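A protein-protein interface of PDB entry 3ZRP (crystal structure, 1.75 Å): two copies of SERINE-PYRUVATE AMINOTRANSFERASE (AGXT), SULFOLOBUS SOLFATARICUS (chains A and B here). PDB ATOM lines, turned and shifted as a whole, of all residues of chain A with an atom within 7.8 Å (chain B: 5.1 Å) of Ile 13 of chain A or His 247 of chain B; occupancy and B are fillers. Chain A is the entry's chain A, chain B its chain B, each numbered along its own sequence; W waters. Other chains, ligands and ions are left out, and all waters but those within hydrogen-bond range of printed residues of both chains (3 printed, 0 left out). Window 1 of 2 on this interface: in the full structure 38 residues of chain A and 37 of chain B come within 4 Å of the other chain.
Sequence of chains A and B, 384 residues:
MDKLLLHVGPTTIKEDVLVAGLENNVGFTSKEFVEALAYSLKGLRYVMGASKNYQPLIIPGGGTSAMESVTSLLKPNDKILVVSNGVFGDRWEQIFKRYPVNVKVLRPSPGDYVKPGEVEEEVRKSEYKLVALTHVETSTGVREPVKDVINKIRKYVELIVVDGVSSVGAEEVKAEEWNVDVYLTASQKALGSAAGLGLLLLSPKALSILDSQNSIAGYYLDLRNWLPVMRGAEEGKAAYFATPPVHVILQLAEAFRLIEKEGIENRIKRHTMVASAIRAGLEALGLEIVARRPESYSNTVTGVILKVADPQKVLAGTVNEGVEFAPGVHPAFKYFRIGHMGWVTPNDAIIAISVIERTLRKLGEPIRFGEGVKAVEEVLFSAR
The backbone carbonyl oxygen (O) of Thr 11 of chain A sits close to the side-chain amide oxygen (OD1) of Asn 24 of chain B (3.4 Å).
The backbone carbonyl oxygen (O) of Thr 11 of chain A sits at hydrogen-bond distance from the backbone NH (N) of Val 26 of chain B, at 3.2 Å.
O of Ile 13 of chain A is in hydrogen-bond range of ND2 of Asn 24 of chain B (2.7 Å).
The side-chain carboxylate of Glu 15 of chain A lies within hydrogen-bond range of the side-chain amide nitrogen of Asn 24 of chain B.
The backbone carbonyl oxygen (O) of Leu 18 of chain A lies within hydrogen-bond range of the side-chain amide nitrogen (NE2) of Gln 251 of chain A, 3.3 Å away.
The backbone carbonyl oxygen (O) of Glu 23 of chain B is in hydrogen-bond range of a ring nitrogen (NE2) of His 247 of chain B (2.9 Å).
The backbone carbonyl oxygen (O) of His 247 of chain B lies close to the side-chain amide oxygen (OE1) of Gln 251 of chain B (3.4 Å).
Among the printed residues, merely in contact across the chains: Thr 12 of chain A with Asn 24 of chain B, Ile 13 of chain A with His 247 of chain B, Leu 18 of chain A with Gly 21 of chain B, Leu 18 of chain A with Leu 22 of chain B, Leu 18 of chain A with Asn 24 of chain B, Val 19 of chain A with Leu 22 of chain B, Ala 195 of chain A with Pro 245 of chain B and Val 248 of chain A with Val 248 of chain B.
Ile 13 of chain A touches just these residues of chain B: Asn 24 (2.7 Å) and His 247 (3.7 Å).
His 247 of chain B touches one residue of chain A.
Of the printed residues of chain A, Asn 24 of chain B touches Thr 11, Thr 12, Ile 13, Glu 15 and Leu 18.
Of the printed residues of chain B, Leu 18 of chain A touches Gly 21, Leu 22 and Asn 24.
Printed residues of chain A within 4 Å of Val 26 of chain B: Thr 11.
Printed residues of chain A within 4 Å of Pro 245 of chain B: Ala 195 (3.7 Å).
Of the printed residues of chain B, Val 19 of chain A touches Leu 22.
The nearest printed residue of chain B that does not touch Ile 13 of chain A is Val 26 of chain B (5.8 Å).
Hydrophobic or aromatic side chains of chain B within 4 Å of the printed part of chain A: Leu 22, Pro 245, His 247 and Val 248.
Among the printed residues, 12 pairs touch across the chains.
Among the printed residues, no Asp or Glu carboxylate lies within 4 Å of a Lys or Arg side-chain nitrogen of the other chain.
Val 248 of chain A touches its own counterpart, Val 248 of chain B.
Positions printed for both chains: 248 and 251.
Of the 12 pairs that touch across the chains among the printed residues, 1 has its exchanged pair printed and touching as well.
Water W1 bridges N of Ala 195 of chain A (2.8 Å) and ND1 of His 247 of chain B (2.8 Å).
Water W3 lies within hydrogen-bond range of the backbone carbonyl oxygen of Gly 21 of chain B (2.8 Å) and the side-chain amide nitrogen of Gln 251 of chain A (2.9 Å).
Water W2 lies within hydrogen-bond range of the backbone carbonyl oxygen (O) of Ala 195 of chain A, the backbone NH (N) of His 247 of chain B and the backbone NH (N) of Val 248 of chain B.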
ATOM      1  N   GLY A   9     -28.180 -32.001  13.695  1.00  0.00           N
ATOM      2  CA  GLY A   9     -27.987 -31.497  15.044  1.00  0.00           C
ATOM      3  C   GLY A   9     -26.753 -32.177  15.605  1.00  0.00           C
ATOM      4  O   GLY A   9     -26.876 -33.059  16.464  1.00  0.00           O
ATOM      5  N   PRO A  10     -25.551 -31.794  15.107  1.00  0.00           N
ATOM      6  CA  PRO A  10     -24.325 -32.403  15.593  1.00  0.00           C
ATOM      7  C   PRO A  10     -24.458 -32.651  17.081  1.00  0.00           C
ATOM      8  O   PRO A  10     -24.841 -31.745  17.826  1.00  0.00           O
ATOM      9  CB  PRO A  10     -23.254 -31.332  15.322  1.00  0.00           C
ATOM     10  CG  PRO A  10     -23.922 -30.246  14.519  1.00  0.00           C
ATOM     11  CD  PRO A  10     -25.262 -30.754  14.105  1.00  0.00           C
ATOM     12  N   THR A  11     -24.189 -33.886  17.495  1.00  0.00           N
ATOM     13  CA  THR A  11     -24.233 -34.251  18.907  1.00  0.00           C
ATOM     14  C   THR A  11     -22.923 -33.874  19.628  1.00  0.00           C
ATOM     15  O   THR A  11     -22.916 -33.715  20.850  1.00  0.00           O
ATOM     16  CB  THR A  11     -24.587 -35.747  19.121  1.00  0.00           C
ATOM     17  OG1 THR A  11     -23.548 -36.575  18.587  1.00  0.00           O
ATOM     18  CG2 THR A  11     -25.925 -36.093  18.453  1.00  0.00           C
ATOM     19  N   THR A  12     -21.837 -33.710  18.867  1.00  0.00           N
ATOM     20  CA  THR A  12     -20.546 -33.270  19.419  1.00  0.00           C
ATOM     21  C   THR A  12     -20.356 -31.758  19.309  1.00  0.00           C
ATOM     22  O   THR A  12     -20.357 -31.185  18.214  1.00  0.00           O
ATOM     23  CB  THR A  12     -19.343 -34.026  18.795  1.00  0.00           C
ATOM     24  OG1 THR A  12     -19.441 -35.416  19.123  1.00  0.00           O
ATOM     25  CG2 THR A  12     -18.010 -33.480  19.326  1.00  0.00           C
ATOM     26  N   ILE A  13     -20.210 -31.131  20.475  1.00  0.00           N
ATOM     27  CA  ILE A  13     -20.022 -29.693  20.603  1.00  0.00           C
ATOM     28  C   ILE A  13     -18.594 -29.472  21.111  1.00  0.00           C
ATOM     29  O   ILE A  13     -18.154 -30.162  22.027  1.00  0.00           O
ATOM     30  CB  ILE A  13     -21.062 -29.079  21.602  1.00  0.00           C
ATOM     31  CG1 ILE A  13     -22.498 -29.323  21.100  1.00  0.00           C
ATOM     32  CG2 ILE A  13     -20.791 -27.591  21.851  1.00  0.00           C
ATOM     33  CD1 ILE A  13     -23.600 -28.865  22.056  1.00  0.00           C
ATOM     34  N   LYS A  14     -17.873 -28.528  20.508  1.00  0.00           N
ATOM     35  CA  LYS A  14     -16.555 -28.151  21.005  1.00  0.00           C
ATOM     36  C   LYS A  14     -16.567 -27.928  22.521  1.00  0.00           C
ATOM     37  O   LYS A  14     -17.513 -27.338  23.065  1.00  0.00           O
ATOM     38  CB  LYS A  14     -16.043 -26.914  20.287  1.00  0.00           C
ATOM     39  CG  LYS A  14     -15.005 -27.239  19.235  1.00  0.00           C
ATOM     40  CD  LYS A  14     -14.369 -25.977  18.700  1.00  0.00           C
ATOM     41  CE  LYS A  14     -12.967 -26.247  18.185  1.00  0.00           C
ATOM     42  NZ  LYS A  14     -12.911 -27.525  17.424  1.00  0.00           N
ATOM     43  N   GLU A  15     -15.531 -28.438  23.187  1.00  0.00           N
ATOM     44  CA  GLU A  15     -15.410 -28.351  24.647  1.00  0.00           C
ATOM     45  C   GLU A  15     -15.388 -26.913  25.140  1.00  0.00           C
ATOM     46  O   GLU A  15     -16.010 -26.603  26.156  1.00  0.00           O
ATOM     47  CB  GLU A  15     -14.174 -29.112  25.154  1.00  0.00           C
ATOM     48  CG  GLU A  15     -14.483 -30.468  25.806  1.00  0.00           C
ATOM     49  CD  GLU A  15     -15.417 -31.316  24.973  1.00  0.00           C
ATOM     50  OE1 GLU A  15     -15.292 -31.286  23.730  1.00  0.00           O
ATOM     51  OE2 GLU A  15     -16.277 -32.009  25.559  1.00  0.00           O
ATOM     52  N   ASP A  16     -14.685 -26.039  24.410  1.00  0.00           N
ATOM     53  CA  ASP A  16     -14.620 -24.613  24.739  1.00  0.00           C
ATOM     54  C   ASP A  16     -16.021 -24.010  24.822  1.00  0.00           C
ATOM     55  O   ASP A  16     -16.276 -23.123  25.639  1.00  0.00           O
ATOM     56  CB  ASP A  16     -13.841 -23.831  23.675  1.00  0.00           C
ATOM     57  CG  ASP A  16     -12.390 -24.236  23.590  1.00  0.00           C
ATOM     58  OD1 ASP A  16     -11.591 -23.773  24.431  1.00  0.00           O
ATOM     59  OD2 ASP A  16     -12.057 -25.006  22.668  1.00  0.00           O
ATOM     60  N   VAL A  17     -16.914 -24.483  23.949  1.00  0.00           N
ATOM     61  CA  VAL A  17     -18.271 -23.941  23.861  1.00  0.00           C
ATOM     62  C   VAL A  17     -19.058 -24.383  25.081  1.00  0.00           C
ATOM     63  O   VAL A  17     -19.638 -23.538  25.769  1.00  0.00           O
ATOM     64  CB  VAL A  17     -18.996 -24.325  22.533  1.00  0.00           C
ATOM     65  CG1 VAL A  17     -20.425 -23.767  22.500  1.00  0.00           C
ATOM     66  CG2 VAL A  17     -18.214 -23.821  21.324  1.00  0.00           C
ATOM     67  N   LEU A  18     -19.050 -25.685  25.371  1.00  0.00           N
ATOM     68  CA  LEU A  18     -19.793 -26.211  26.533  1.00  0.00           C
ATOM     69  C   LEU A  18     -19.319 -25.628  27.858  1.00  0.00           C
ATOM     70  O   LEU A  18     -20.139 -25.321  28.731  1.00  0.00           O
ATOM     71  CB  LEU A  18     -19.717 -27.731  26.601  1.00  0.00           C
ATOM     72  CG  LEU A  18     -20.462 -28.536  25.547  1.00  0.00           C
ATOM     73  CD1 LEU A  18     -20.017 -29.982  25.684  1.00  0.00           C
ATOM     74  CD2 LEU A  18     -21.985 -28.383  25.687  1.00  0.00           C
ATOM     75  N   VAL A  19     -17.998 -25.485  27.998  1.00  0.00           N
ATOM     76  CA  VAL A  19     -17.383 -24.985  29.223  1.00  0.00           C
ATOM     77  C   VAL A  19     -17.791 -23.541  29.492  1.00  0.00           C
ATOM     78  O   VAL A  19     -17.955 -23.148  30.655  1.00  0.00           O
ATOM     79  CB  VAL A  19     -15.821 -25.130  29.198  1.00  0.00           C
ATOM     80  CG1 VAL A  19     -15.176 -24.273  30.275  1.00  0.00           C
ATOM     81  CG2 VAL A  19     -15.422 -26.580  29.410  1.00  0.00           C
ATOM     82  N   SER A 187     -29.306 -22.280  17.119  1.00  0.00           N
ATOM     83  CA  SER A 187     -27.995 -22.346  17.749  1.00  0.00           C
ATOM     84  C   SER A 187     -27.224 -23.659  17.524  1.00  0.00           C
ATOM     85  O   SER A 187     -25.991 -23.681  17.534  1.00  0.00           O
ATOM     86  CB  SER A 187     -28.085 -21.977  19.235  1.00  0.00           C
ATOM     87  OG  SER A 187     -29.053 -22.741  19.929  1.00  0.00           O
ATOM     88  N   GLN A 188     -27.953 -24.746  17.310  1.00  0.00           N
ATOM     89  CA  GLN A 188     -27.372 -26.085  17.430  1.00  0.00           C
ATOM     90  C   GLN A 188     -26.956 -26.759  16.133  1.00  0.00           C
ATOM     91  O   GLN A 188     -26.560 -27.941  16.163  1.00  0.00           O
ATOM     92  CB  GLN A 188     -28.336 -27.030  18.201  1.00  0.00           C
ATOM     93  CG  GLN A 188     -29.562 -27.595  17.407  1.00  0.00           C
ATOM     94  CD  GLN A 188     -30.700 -26.569  17.146  1.00  0.00           C
ATOM     95  OE1 GLN A 188     -30.650 -25.411  17.593  1.00  0.00           O
ATOM     96  NE2 GLN A 188     -31.694 -26.985  16.362  1.00  0.00           N
ATOM     97  N   LEU A 191     -23.718 -23.612  13.367  1.00  0.00           N
ATOM     98  CA  LEU A 191     -23.051 -22.760  14.353  1.00  0.00           C
ATOM     99  C   LEU A 191     -22.395 -23.613  15.432  1.00  0.00           C
ATOM    100  O   LEU A 191     -21.455 -23.170  16.089  1.00  0.00           O
ATOM    101  CB  LEU A 191     -24.025 -21.752  14.979  1.00  0.00           C
ATOM    102  CG  LEU A 191     -24.664 -20.776  13.986  1.00  0.00           C
ATOM    103  CD1 LEU A 191     -25.687 -19.881  14.664  1.00  0.00           C
ATOM    104  CD2 LEU A 191     -23.581 -19.912  13.249  1.00  0.00           C
ATOM    105  N   GLY A 192     -22.897 -24.842  15.605  1.00  0.00           N
ATOM    106  CA  GLY A 192     -22.256 -25.835  16.496  1.00  0.00           C
ATOM    107  C   GLY A 192     -22.289 -25.467  17.973  1.00  0.00           C
ATOM    108  O   GLY A 192     -21.353 -25.778  18.709  1.00  0.00           O
ATOM    109  N   SER A 193     -23.366 -24.813  18.423  1.00  0.00           N
ATOM    110  CA  SER A 193     -23.500 -24.470  19.849  1.00  0.00           C
ATOM    111  C   SER A 193     -24.611 -25.297  20.508  1.00  0.00           C
ATOM    112  O   SER A 193     -25.210 -26.176  19.878  1.00  0.00           O
ATOM    113  CB  SER A 193     -23.772 -22.987  20.016  1.00  0.00           C
ATOM    114  OG  SER A 193     -23.652 -22.645  21.385  1.00  0.00           O
ATOM    115  N   ALA A 194     -24.884 -25.042  21.780  1.00  0.00           N
ATOM    116  CA  ALA A 194     -25.932 -25.822  22.467  1.00  0.00           C
ATOM    117  C   ALA A 194     -27.335 -25.386  21.988  1.00  0.00           C
ATOM    118  O   ALA A 194     -27.537 -24.223  21.646  1.00  0.00           O
ATOM    119  CB  ALA A 194     -25.800 -25.656  23.976  1.00  0.00           C
ATOM    120  N   ALA A 195     -28.297 -26.315  22.000  1.00  0.00           N
ATOM    121  CA  ALA A 195     -29.676 -26.064  21.557  1.00  0.00           C
ATOM    122  C   ALA A 195     -30.454 -25.180  22.523  1.00  0.00           C
ATOM    123  O   ALA A 195     -30.126 -25.138  23.726  1.00  0.00           O
ATOM    124  CB  ALA A 195     -30.425 -27.404  21.358  1.00  0.00           C
ATOM    125  N   GLY A 196     -31.459 -24.459  21.997  1.00  0.00           N
ATOM    126  CA  GLY A 196     -32.335 -23.618  22.834  1.00  0.00           C
ATOM    127  C   GLY A 196     -32.587 -22.189  22.368  1.00  0.00           C
ATOM    128  O   GLY A 196     -33.336 -21.452  23.008  1.00  0.00           O
ATOM    129  N   VAL A 248     -27.151 -20.808  27.707  1.00  0.00           N
ATOM    130  CA  VAL A 248     -27.113 -21.204  26.294  1.00  0.00           C
ATOM    131  C   VAL A 248     -26.552 -20.034  25.470  1.00  0.00           C
ATOM    132  O   VAL A 248     -25.837 -20.237  24.498  1.00  0.00           O
ATOM    133  CB  VAL A 248     -28.524 -21.607  25.795  1.00  0.00           C
ATOM    134  CG1 VAL A 248     -28.522 -21.948  24.311  1.00  0.00           C
ATOM    135  CG2 VAL A 248     -28.995 -22.810  26.575  1.00  0.00           C
ATOM    136  N   GLN A 251     -22.774 -19.836  25.912  1.00  0.00           N
ATOM    137  CA  GLN A 251     -22.190 -20.828  25.008  1.00  0.00           C
ATOM    138  C   GLN A 251     -22.175 -20.309  23.559  1.00  0.00           C
ATOM    139  O   GLN A 251     -21.158 -20.434  22.859  1.00  0.00           O
ATOM    140  CB  GLN A 251     -22.914 -22.185  25.135  1.00  0.00           C
ATOM    141  CG  GLN A 251     -22.689 -22.843  26.500  1.00  0.00           C
ATOM    142  CD  GLN A 251     -23.652 -23.984  26.830  1.00  0.00           C
ATOM    143  OE1 GLN A 251     -24.862 -23.860  26.671  1.00  0.00           O
ATOM    144  NE2 GLN A 251     -23.112 -25.086  27.334  1.00  0.00           N
ATOM    145  N   ALA A 255     -19.155 -19.832  20.786  1.00  0.00           N
ATOM    146  CA  ALA A 255     -19.187 -20.376  19.418  1.00  0.00           C
ATOM    147  C   ALA A 255     -18.864 -19.275  18.405  1.00  0.00           C
ATOM    148  O   ALA A 255     -18.038 -19.474  17.498  1.00  0.00           O
ATOM    149  CB  ALA A 255     -20.539 -21.033  19.102  1.00  0.00           C
ATOM    150  N   TRP A 343     -18.188 -28.183  13.226  1.00  0.00           N
ATOM    151  CA  TRP A 343     -16.736 -28.323  13.400  1.00  0.00           C
ATOM    152  C   TRP A 343     -16.143 -29.519  12.684  1.00  0.00           C
ATOM    153  O   TRP A 343     -15.028 -29.948  12.974  1.00  0.00           O
ATOM    154  CB  TRP A 343     -16.333 -28.233  14.886  1.00  0.00           C
ATOM    155  CG  TRP A 343     -16.448 -26.786  15.359  1.00  0.00           C
ATOM    156  CD1 TRP A 343     -17.471 -26.233  16.081  1.00  0.00           C
ATOM    157  CD2 TRP A 343     -15.551 -25.710  15.045  1.00  0.00           C
ATOM    158  NE1 TRP A 343     -17.234 -24.893  16.288  1.00  0.00           N
ATOM    159  CE2 TRP A 343     -16.068 -24.545  15.655  1.00  0.00           C
ATOM    160  CE3 TRP A 343     -14.343 -25.625  14.329  1.00  0.00           C
ATOM    161  CZ2 TRP A 343     -15.424 -23.306  15.566  1.00  0.00           C
ATOM    162  CZ3 TRP A 343     -13.699 -24.395  14.247  1.00  0.00           C
ATOM    163  CH2 TRP A 343     -14.243 -23.253  14.857  1.00  0.00           C
ATOM    164  N   GLY B  21     -24.522 -30.359  32.593  1.00  0.00           N
ATOM    165  CA  GLY B  21     -24.675 -29.865  31.220  1.00  0.00           C
ATOM    166  C   GLY B  21     -23.421 -29.979  30.366  1.00  0.00           C
ATOM    167  O   GLY B  21     -23.420 -29.552  29.200  1.00  0.00           O
ATOM    168  N   LEU B  22     -22.350 -30.543  30.928  1.00  0.00           N
ATOM    169  CA  LEU B  22     -21.107 -30.720  30.163  1.00  0.00           C
ATOM    170  C   LEU B  22     -21.053 -32.009  29.347  1.00  0.00           C
ATOM    171  O   LEU B  22     -20.134 -32.194  28.549  1.00  0.00           O
ATOM    172  CB  LEU B  22     -19.861 -30.602  31.051  1.00  0.00           C
ATOM    173  CG  LEU B  22     -19.470 -29.234  31.609  1.00  0.00           C
ATOM    174  CD1 LEU B  22     -18.184 -29.367  32.407  1.00  0.00           C
ATOM    175  CD2 LEU B  22     -19.339 -28.158  30.510  1.00  0.00           C
ATOM    176  N   GLU B  23     -22.033 -32.889  29.549  1.00  0.00           N
ATOM    177  CA  GLU B  23     -22.125 -34.147  28.800  1.00  0.00           C
ATOM    178  C   GLU B  23     -22.127 -33.901  27.298  1.00  0.00           C
ATOM    179  O   GLU B  23     -22.996 -33.199  26.779  1.00  0.00           O
ATOM    180  CB  GLU B  23     -23.372 -34.940  29.206  1.00  0.00           C
ATOM    181  CG  GLU B  23     -23.273 -35.575  30.581  1.00  0.00           C
ATOM    182  CD  GLU B  23     -22.225 -36.664  30.673  1.00  0.00           C
ATOM    183  OE1 GLU B  23     -22.312 -37.644  29.907  1.00  0.00           O
ATOM    184  OE2 GLU B  23     -21.315 -36.543  31.521  1.00  0.00           O
ATOM    185  N   ASN B  24     -21.142 -34.470  26.601  1.00  0.00           N
ATOM    186  CA  ASN B  24     -21.021 -34.295  25.156  1.00  0.00           C
ATOM    187  C   ASN B  24     -21.573 -35.491  24.367  1.00  0.00           C
ATOM    188  O   ASN B  24     -21.969 -36.500  24.971  1.00  0.00           O
ATOM    189  CB  ASN B  24     -19.571 -34.002  24.774  1.00  0.00           C
ATOM    190  CG  ASN B  24     -19.459 -32.970  23.674  1.00  0.00           C
ATOM    191  OD1 ASN B  24     -20.346 -32.843  22.819  1.00  0.00           O
ATOM    192  ND2 ASN B  24     -18.362 -32.223  23.686  1.00  0.00           N
ATOM    193  N   VAL B  26     -24.395 -35.779  22.802  1.00  0.00           N
ATOM    194  CA  VAL B  26     -25.787 -35.999  23.195  1.00  0.00           C
ATOM    195  C   VAL B  26     -26.710 -35.106  22.374  1.00  0.00           C
ATOM    196  O   VAL B  26     -26.528 -33.882  22.328  1.00  0.00           O
ATOM    197  CB  VAL B  26     -25.997 -35.743  24.727  1.00  0.00           C
ATOM    198  CG1 VAL B  26     -27.478 -35.730  25.092  1.00  0.00           C
ATOM    199  CG2 VAL B  26     -25.258 -36.787  25.566  1.00  0.00           C
ATOM    200  N   PRO B 245     -34.181 -27.774  24.427  1.00  0.00           N
ATOM    201  CA  PRO B 245     -32.862 -27.372  24.934  1.00  0.00           C
ATOM    202  C   PRO B 245     -32.199 -28.573  25.646  1.00  0.00           C
ATOM    203  O   PRO B 245     -32.308 -28.738  26.862  1.00  0.00           O
ATOM    204  CB  PRO B 245     -33.180 -26.212  25.889  1.00  0.00           C
ATOM    205  CG  PRO B 245     -34.642 -25.806  25.551  1.00  0.00           C
ATOM    206  CD  PRO B 245     -35.265 -27.101  25.165  1.00  0.00           C
ATOM    207  N   VAL B 246     -31.519 -29.397  24.861  1.00  0.00           N
ATOM    208  CA  VAL B 246     -31.006 -30.709  25.280  1.00  0.00           C
ATOM    209  C   VAL B 246     -30.187 -30.643  26.586  1.00  0.00           C
ATOM    210  O   VAL B 246     -30.497 -31.346  27.557  1.00  0.00           O
ATOM    211  CB  VAL B 246     -30.230 -31.409  24.092  1.00  0.00           C
ATOM    212  CG1 VAL B 246     -29.405 -32.603  24.556  1.00  0.00           C
ATOM    213  CG2 VAL B 246     -31.207 -31.840  22.994  1.00  0.00           C
ATOM    214  N   HIS B 247     -29.167 -29.786  26.614  1.00  0.00           N
ATOM    215  CA  HIS B 247     -28.291 -29.686  27.778  1.00  0.00           C
ATOM    216  C   HIS B 247     -28.946 -29.003  28.987  1.00  0.00           C
ATOM    217  O   HIS B 247     -28.596 -29.290  30.132  1.00  0.00           O
ATOM    218  CB  HIS B 247     -26.953 -29.039  27.392  1.00  0.00           C
ATOM    219  CG  HIS B 247     -26.140 -29.892  26.460  1.00  0.00           C
ATOM    220  ND1 HIS B 247     -26.359 -29.916  25.099  1.00  0.00           N
ATOM    221  CD2 HIS B 247     -25.135 -30.773  26.696  1.00  0.00           C
ATOM    222  CE1 HIS B 247     -25.513 -30.763  24.532  1.00  0.00           C
ATOM    223  NE2 HIS B 247     -24.766 -31.302  25.480  1.00  0.00           N
ATOM    224  N   VAL B 248     -29.911 -28.122  28.730  1.00  0.00           N
ATOM    225  CA  VAL B 248     -30.683 -27.500  29.807  1.00  0.00           C
ATOM    226  C   VAL B 248     -31.533 -28.585  30.505  1.00  0.00           C
ATOM    227  O   VAL B 248     -31.737 -28.554  31.708  1.00  0.00           O
ATOM    228  CB  VAL B 248     -31.579 -26.361  29.264  1.00  0.00           C
ATOM    229  CG1 VAL B 248     -32.441 -25.745  30.389  1.00  0.00           C
ATOM    230  CG2 VAL B 248     -30.701 -25.274  28.690  1.00  0.00           C
ATOM    231  N   ILE B 249     -32.030 -29.523  29.721  1.00  0.00           N
ATOM    232  CA  ILE B 249     -32.839 -30.638  30.255  1.00  0.00           C
ATOM    233  C   ILE B 249     -31.970 -31.641  31.049  1.00  0.00           C
ATOM    234  O   ILE B 249     -32.435 -32.236  32.035  1.00  0.00           O
ATOM    235  CB  ILE B 249     -33.642 -31.347  29.149  1.00  0.00           C
ATOM    236  CG1 ILE B 249     -34.769 -30.433  28.638  1.00  0.00           C
ATOM    237  CG2 ILE B 249     -34.260 -32.658  29.657  1.00  0.00           C
ATOM    238  CD1 ILE B 249     -35.415 -30.860  27.338  1.00  0.00           C
ATOM    239  N   LEU B 250     -30.727 -31.840  30.614  1.00  0.00           N
ATOM    240  CA  LEU B 250     -29.760 -32.642  31.397  1.00  0.00           C
ATOM    241  C   LEU B 250     -29.530 -32.015  32.767  1.00  0.00           C
ATOM    242  O   LEU B 250     -29.522 -32.712  33.792  1.00  0.00           O
ATOM    243  CB  LEU B 250     -28.416 -32.761  30.651  1.00  0.00           C
ATOM    244  CG  LEU B 250     -28.366 -33.527  29.325  1.00  0.00           C
ATOM    245  CD1 LEU B 250     -26.935 -33.565  28.813  1.00  0.00           C
ATOM    246  CD2 LEU B 250     -28.879 -34.948  29.545  1.00  0.00           C
ATOM    247  N   GLN B 251     -29.325 -30.698  32.773  1.00  0.00           N
ATOM    248  CA  GLN B 251     -29.159 -29.949  34.021  1.00  0.00           C
ATOM    249  C   GLN B 251     -30.416 -30.089  34.901  1.00  0.00           C
ATOM    250  O   GLN B 251     -30.304 -30.333  36.106  1.00  0.00           O
ATOM    251  CB  GLN B 251     -28.800 -28.482  33.745  1.00  0.00           C
ATOM    252  CG  GLN B 251     -27.418 -28.323  33.118  1.00  0.00           C
ATOM    253  CD  GLN B 251     -27.162 -26.943  32.503  1.00  0.00           C
ATOM    254  OE1 GLN B 251     -27.990 -26.414  31.752  1.00  0.00           O
ATOM    255  NE2 GLN B 251     -25.998 -26.378  32.789  1.00  0.00           N
HETATM  256  O   HOH W   1     -28.027 -28.868  23.078  1.00  0.00           O
HETATM  257  O   HOH W   2     -29.063 -26.806  25.855  1.00  0.00           O
HETATM  258  O   HOH W   3     -24.632 -27.024  28.889  1.00  0.00           O
